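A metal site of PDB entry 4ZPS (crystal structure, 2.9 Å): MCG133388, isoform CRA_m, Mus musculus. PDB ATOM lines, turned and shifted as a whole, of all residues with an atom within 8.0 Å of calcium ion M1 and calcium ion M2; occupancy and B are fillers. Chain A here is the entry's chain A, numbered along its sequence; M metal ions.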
ATOM      1  N   PRO A   7      12.134 -24.032  14.361  1.00  0.00           N
ATOM      2  CA  PRO A   7      11.188 -23.309  15.208  1.00  0.00           C
ATOM      3  C   PRO A   7      11.253 -21.796  14.991  1.00  0.00           C
ATOM      4  O   PRO A   7      12.288 -21.277  14.583  1.00  0.00           O
ATOM      5  CB  PRO A   7      11.635 -23.670  16.626  1.00  0.00           C
ATOM      6  CG  PRO A   7      12.320 -24.980  16.478  1.00  0.00           C
ATOM      7  CD  PRO A   7      13.010 -24.918  15.156  1.00  0.00           C
ATOM      8  N   GLU A   8      10.140 -21.109  15.260  1.00  0.00           N
ATOM      9  CA  GLU A   8      10.088 -19.666  15.113  1.00  0.00           C
ATOM     10  C   GLU A   8      10.666 -18.958  16.331  1.00  0.00           C
ATOM     11  O   GLU A   8      11.004 -19.605  17.319  1.00  0.00           O
ATOM     12  CB  GLU A   8       8.638 -19.206  14.887  1.00  0.00           C
ATOM     13  CG  GLU A   8       7.741 -19.430  16.083  1.00  0.00           C
ATOM     14  CD  GLU A   8       6.319 -18.975  15.840  1.00  0.00           C
ATOM     15  OE1 GLU A   8       6.022 -18.504  14.721  1.00  0.00           O
ATOM     16  OE2 GLU A   8       5.488 -19.083  16.764  1.00  0.00           O
ATOM     17  N   GLU A   9      10.776 -17.631  16.243  1.00  0.00           N
ATOM     18  CA  GLU A   9      11.259 -16.796  17.344  1.00  0.00           C
ATOM     19  C   GLU A   9      12.601 -17.250  17.899  1.00  0.00           C
ATOM     20  O   GLU A   9      12.936 -16.972  19.045  1.00  0.00           O
ATOM     21  CB  GLU A   9      10.221 -16.742  18.468  1.00  0.00           C
ATOM     22  N   THR A  10      13.370 -17.961  17.069  1.00  0.00           N
ATOM     23  CA  THR A  10      14.659 -18.491  17.492  1.00  0.00           C
ATOM     24  C   THR A  10      15.747 -17.429  17.379  1.00  0.00           C
ATOM     25  O   THR A  10      15.522 -16.366  16.814  1.00  0.00           O
ATOM     26  CB  THR A  10      15.056 -19.728  16.656  1.00  0.00           C
ATOM     27  OG1 THR A  10      16.288 -20.266  17.142  1.00  0.00           O
ATOM     28  CG2 THR A  10      15.211 -19.359  15.192  1.00  0.00           C
ATOM     29  N   ARG A  60      15.662 -12.491  12.896  1.00  0.00           N
ATOM     30  CA  ARG A  60      14.432 -12.865  13.585  1.00  0.00           C
ATOM     31  C   ARG A  60      13.482 -13.622  12.656  1.00  0.00           C
ATOM     32  O   ARG A  60      13.256 -13.206  11.526  1.00  0.00           O
ATOM     33  CB  ARG A  60      13.722 -11.621  14.132  1.00  0.00           C
ATOM     34  CG  ARG A  60      12.436 -11.933  14.879  1.00  0.00           C
ATOM     35  CD  ARG A  60      11.368 -10.874  14.642  1.00  0.00           C
ATOM     36  NE  ARG A  60      10.076 -11.282  15.169  1.00  0.00           N
ATOM     37  CZ  ARG A  60       8.949 -10.607  14.994  1.00  0.00           C
ATOM     38  NH1 ARG A  60       8.939  -9.487  14.290  1.00  0.00           N
ATOM     39  NH2 ARG A  60       7.822 -11.062  15.522  1.00  0.00           N
ATOM     40  N   ILE A  61      12.950 -14.735  13.146  1.00  0.00           N
ATOM     41  CA  ILE A  61      12.021 -15.543  12.356  1.00  0.00           C
ATOM     42  C   ILE A  61      10.701 -15.739  13.101  1.00  0.00           C
ATOM     43  O   ILE A  61      10.654 -16.373  14.152  1.00  0.00           O
ATOM     44  CB  ILE A  61      12.618 -16.930  12.035  1.00  0.00           C
ATOM     45  CG1 ILE A  61      13.939 -16.780  11.279  1.00  0.00           C
ATOM     46  CG2 ILE A  61      11.636 -17.759  11.222  1.00  0.00           C
ATOM     47  CD1 ILE A  61      14.561 -18.088  10.865  1.00  0.00           C
ATOM     48  N   ASP A  62       9.628 -15.190  12.539  1.00  0.00           N
ATOM     49  CA  ASP A  62       8.307 -15.341  13.122  1.00  0.00           C
ATOM     50  C   ASP A  62       7.262 -15.642  12.050  1.00  0.00           C
ATOM     51  O   ASP A  62       7.139 -14.893  11.073  1.00  0.00           O
ATOM     52  CB  ASP A  62       7.912 -14.089  13.912  1.00  0.00           C
ATOM     53  CG  ASP A  62       7.242 -14.426  15.237  1.00  0.00           C
ATOM     54  OD1 ASP A  62       7.630 -15.437  15.853  1.00  0.00           O
ATOM     55  OD2 ASP A  62       6.344 -13.673  15.655  1.00  0.00           O
ATOM     56  N   ARG A  63       6.515 -16.725  12.233  1.00  0.00           N
ATOM     57  CA  ARG A  63       5.521 -17.171  11.260  1.00  0.00           C
ATOM     58  C   ARG A  63       4.389 -16.161  11.081  1.00  0.00           C
ATOM     59  O   ARG A  63       3.834 -16.017   9.994  1.00  0.00           O
ATOM     60  CB  ARG A  63       4.956 -18.536  11.688  1.00  0.00           C
ATOM     61  CG  ARG A  63       3.713 -18.975  10.935  1.00  0.00           C
ATOM     62  CD  ARG A  63       3.318 -20.393  11.289  1.00  0.00           C
ATOM     63  NE  ARG A  63       1.912 -20.665  10.989  1.00  0.00           N
ATOM     64  CZ  ARG A  63       1.342 -21.860  11.070  1.00  0.00           C
ATOM     65  NH1 ARG A  63       2.067 -22.920  11.427  1.00  0.00           N
ATOM     66  NH2 ARG A  63       0.058 -22.013  10.786  1.00  0.00           N
ATOM     67  N   GLU A  64       4.064 -15.443  12.159  1.00  0.00           N
ATOM     68  CA  GLU A  64       2.960 -14.481  12.143  1.00  0.00           C
ATOM     69  C   GLU A  64       3.171 -13.374  11.104  1.00  0.00           C
ATOM     70  O   GLU A  64       2.215 -12.915  10.475  1.00  0.00           O
ATOM     71  CB  GLU A  64       2.778 -13.853  13.534  1.00  0.00           C
ATOM     72  CG  GLU A  64       2.135 -14.777  14.552  1.00  0.00           C
ATOM     73  CD  GLU A  64       3.042 -15.915  14.974  1.00  0.00           C
ATOM     74  OE1 GLU A  64       3.974 -15.664  15.770  1.00  0.00           O
ATOM     75  OE2 GLU A  64       2.824 -17.056  14.512  1.00  0.00           O
ATOM     76  N   GLU A  65       4.421 -12.957  10.923  1.00  0.00           N
ATOM     77  CA  GLU A  65       4.746 -11.902   9.972  1.00  0.00           C
ATOM     78  C   GLU A  65       5.161 -12.495   8.639  1.00  0.00           C
ATOM     79  O   GLU A  65       5.143 -11.810   7.610  1.00  0.00           O
ATOM     80  CB  GLU A  65       5.838 -10.999  10.530  1.00  0.00           C
ATOM     81  CG  GLU A  65       6.059  -9.710   9.744  1.00  0.00           C
ATOM     82  CD  GLU A  65       7.101  -8.812  10.372  1.00  0.00           C
ATOM     83  OE1 GLU A  65       7.575  -9.134  11.473  1.00  0.00           O
ATOM     84  OE2 GLU A  65       7.450  -7.782   9.750  1.00  0.00           O
ATOM     85  N   ALA A  68       1.678 -16.459   8.823  1.00  0.00           N
ATOM     86  CA  ALA A  68       0.447 -16.214   9.558  1.00  0.00           C
ATOM     87  C   ALA A  68      -0.606 -17.288   9.336  1.00  0.00           C
ATOM     88  O   ALA A  68      -0.535 -18.376   9.924  1.00  0.00           O
ATOM     89  CB  ALA A  68      -0.121 -14.838   9.203  1.00  0.00           C
ATOM     90  N   ILE A  94       8.806 -23.889   8.951  1.00  0.00           N
ATOM     91  CA  ILE A  94       8.896 -23.106  10.179  1.00  0.00           C
ATOM     92  C   ILE A  94       7.840 -23.550  11.199  1.00  0.00           C
ATOM     93  O   ILE A  94       6.634 -23.503  10.914  1.00  0.00           O
ATOM     94  CB  ILE A  94       8.746 -21.597   9.916  1.00  0.00           C
ATOM     95  CG1 ILE A  94       9.871 -21.108   8.989  1.00  0.00           C
ATOM     96  CG2 ILE A  94       8.749 -20.818  11.225  1.00  0.00           C
ATOM     97  CD1 ILE A  94       9.803 -19.627   8.686  1.00  0.00           C
ATOM     98  N   THR A  95       8.295 -23.963  12.375  1.00  0.00           N
ATOM     99  CA  THR A  95       7.384 -24.447  13.418  1.00  0.00           C
ATOM    100  C   THR A  95       6.699 -23.283  14.133  1.00  0.00           C
ATOM    101  O   THR A  95       7.348 -22.334  14.552  1.00  0.00           O
ATOM    102  CB  THR A  95       8.133 -25.314  14.455  1.00  0.00           C
ATOM    103  OG1 THR A  95       8.722 -26.447  13.797  1.00  0.00           O
ATOM    104  CG2 THR A  95       7.186 -25.805  15.533  1.00  0.00           C
ATOM    105  N   ASP A  96       5.373 -23.373  14.254  1.00  0.00           N
ATOM    106  CA  ASP A  96       4.595 -22.370  14.970  1.00  0.00           C
ATOM    107  C   ASP A  96       4.651 -22.606  16.468  1.00  0.00           C
ATOM    108  O   ASP A  96       4.488 -23.737  16.935  1.00  0.00           O
ATOM    109  CB  ASP A  96       3.131 -22.385  14.484  1.00  0.00           C
ATOM    110  CG  ASP A  96       2.260 -21.381  15.217  1.00  0.00           C
ATOM    111  OD1 ASP A  96       1.741 -21.712  16.305  1.00  0.00           O
ATOM    112  OD2 ASP A  96       2.071 -20.264  14.698  1.00  0.00           O
ATOM    113  N   ILE A  97       4.894 -21.544  17.220  1.00  0.00           N
ATOM    114  CA  ILE A  97       4.895 -21.613  18.682  1.00  0.00           C
ATOM    115  C   ILE A  97       3.804 -20.708  19.237  1.00  0.00           C
ATOM    116  O   ILE A  97       3.265 -19.859  18.524  1.00  0.00           O
ATOM    117  CB  ILE A  97       6.254 -21.212  19.268  1.00  0.00           C
ATOM    118  N   ASN A  98       3.476 -20.890  20.515  1.00  0.00           N
ATOM    119  CA  ASN A  98       2.434 -20.095  21.152  1.00  0.00           C
ATOM    120  C   ASN A  98       2.989 -18.838  21.804  1.00  0.00           C
ATOM    121  O   ASN A  98       3.446 -18.869  22.943  1.00  0.00           O
ATOM    122  CB  ASN A  98       1.689 -20.931  22.187  1.00  0.00           C
ATOM    123  CG  ASN A  98       0.322 -20.379  22.515  1.00  0.00           C
ATOM    124  OD1 ASN A  98       0.040 -19.205  22.278  1.00  0.00           O
ATOM    125  ND2 ASN A  98      -0.551 -21.218  23.059  1.00  0.00           N
ATOM    126  N   ASP A  99       2.964 -17.733  21.060  1.00  0.00           N
ATOM    127  CA  ASP A  99       3.431 -16.444  21.585  1.00  0.00           C
ATOM    128  C   ASP A  99       2.433 -15.343  21.267  1.00  0.00           C
ATOM    129  O   ASP A  99       2.716 -14.156  21.464  1.00  0.00           O
ATOM    130  CB  ASP A  99       4.806 -16.102  21.018  1.00  0.00           C
ATOM    131  CG  ASP A  99       4.801 -16.013  19.499  1.00  0.00           C
ATOM    132  OD1 ASP A  99       4.089 -16.799  18.847  1.00  0.00           O
ATOM    133  OD2 ASP A  99       5.508 -15.134  18.960  1.00  0.00           O
ATOM    134  N   ASN A 100       1.267 -15.740  20.756  1.00  0.00           N
ATOM    135  CA  ASN A 100       0.229 -14.778  20.393  1.00  0.00           C
ATOM    136  C   ASN A 100      -1.170 -15.292  20.737  1.00  0.00           C
ATOM    137  O   ASN A 100      -1.833 -15.931  19.922  1.00  0.00           O
ATOM    138  CB  ASN A 100       0.319 -14.459  18.900  1.00  0.00           C
ATOM    139  N   PRO A 131      -3.489 -14.861  15.966  1.00  0.00           N
ATOM    140  CA  PRO A 131      -2.383 -14.778  15.008  1.00  0.00           C
ATOM    141  C   PRO A 131      -1.813 -16.145  14.676  1.00  0.00           C
ATOM    142  O   PRO A 131      -1.498 -16.425  13.513  1.00  0.00           O
ATOM    143  CB  PRO A 131      -1.353 -13.906  15.734  1.00  0.00           C
ATOM    144  CG  PRO A 131      -2.164 -13.090  16.684  1.00  0.00           C
ATOM    145  CD  PRO A 131      -3.274 -13.997  17.141  1.00  0.00           C
ATOM    146  N   ASP A 132      -1.674 -16.994  15.689  1.00  0.00           N
ATOM    147  CA  ASP A 132      -1.233 -18.367  15.495  1.00  0.00           C
ATOM    148  C   ASP A 132      -2.404 -19.217  14.994  1.00  0.00           C
ATOM    149  O   ASP A 132      -3.560 -18.892  15.272  1.00  0.00           O
ATOM    150  CB  ASP A 132      -0.659 -18.944  16.778  1.00  0.00           C
ATOM    151  CG  ASP A 132       0.113 -17.925  17.588  1.00  0.00           C
ATOM    152  OD1 ASP A 132       0.718 -17.012  16.974  1.00  0.00           O
ATOM    153  OD2 ASP A 132       0.111 -18.020  18.825  1.00  0.00           O
ATOM    154  N   VAL A 133      -2.098 -20.284  14.271  1.00  0.00           N
ATOM    155  CA  VAL A 133      -3.143 -21.152  13.736  1.00  0.00           C
ATOM    156  C   VAL A 133      -2.907 -22.601  14.166  1.00  0.00           C
ATOM    157  O   VAL A 133      -1.757 -23.063  14.230  1.00  0.00           O
ATOM    158  CB  VAL A 133      -3.201 -21.084  12.193  1.00  0.00           C
ATOM    159  CG1 VAL A 133      -4.403 -21.848  11.668  1.00  0.00           C
ATOM    160  CG2 VAL A 133      -3.252 -19.635  11.729  1.00  0.00           C
ATOM    161  N   ASN A 136      -2.613 -23.809  18.734  1.00  0.00           N
ATOM    162  CA  ASN A 136      -2.192 -22.546  19.317  1.00  0.00           C
ATOM    163  C   ASN A 136      -3.024 -21.379  18.813  1.00  0.00           C
ATOM    164  O   ASN A 136      -2.589 -20.230  18.849  1.00  0.00           O
ATOM    165  CB  ASN A 136      -0.709 -22.294  19.039  1.00  0.00           C
ATOM    166  CG  ASN A 136       0.171 -23.419  19.525  1.00  0.00           C
ATOM    167  OD1 ASN A 136       0.491 -23.514  20.704  1.00  0.00           O
ATOM    168  ND2 ASN A 136       0.585 -24.276  18.598  1.00  0.00           N
HETATM  169 CA    CA M   1       3.204 -18.785  16.209  1.00  0.00          CA
HETATM  170 CA    CA M   2       5.846 -16.612  17.046  1.00  0.00          CA
HETATM  171 CA    CA M   3      -1.882 -18.202  20.914  1.00  0.00          CA
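Calcium ion M2 is bound by OD2 of Asp 99 (2.4 Å), OD1 of Asp 62 (2.4 Å), OE1 of Glu 64 (2.5 Å), OE2 of Glu 8 (2.5 Å) and OD1 of Asp 99 (2.5 Å). Calcium ion M2 has five donor atoms within binding distance. Slightly farther from calcium ion M2 lies OE1 of Glu 8 (3.0 Å).
Along chain A the residues within 4 Å of calcium ion M2 span positions 8 to 99. The nearest printed residue that does not touch calcium ion M2 is Ile 97 (4.4 Å).
The side-chain carboxylate (OE2) of Glu 8 is bound to calcium ion M1, at 2.4 Å. Calcium ion M1 is bound by OD2 of Asp 96. Calcium ion M1 is bound by OE2 of Glu 64, at 2.5 Å. O of Ile 97 binds calcium ion M1, at 2.6 Å. Calcium ion M1 has four donor atoms within binding distance. Slightly farther from calcium ion M1 lies the side-chain carboxylate (OD1) of Asp 132 (3.1 Å).
The side-chain carboxylate of Glu 8 is in hydrogen-bond range of the backbone NH of Arg 63, at 3.1 Å. N of Glu 8 is in hydrogen-bond range of O of Thr 95 (3.1 Å). The side-chain carboxylate (OD2) of Asp 96 lies close to the guanidinium group (NE) of Arg 63, at 3.7 Å. OD2 of Asp 62 lies within salt-bridge range of NH2 of Arg 60 (3.0 Å).
Of the 22 residues printed, 6 come within 4 Å of calcium ion M1.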
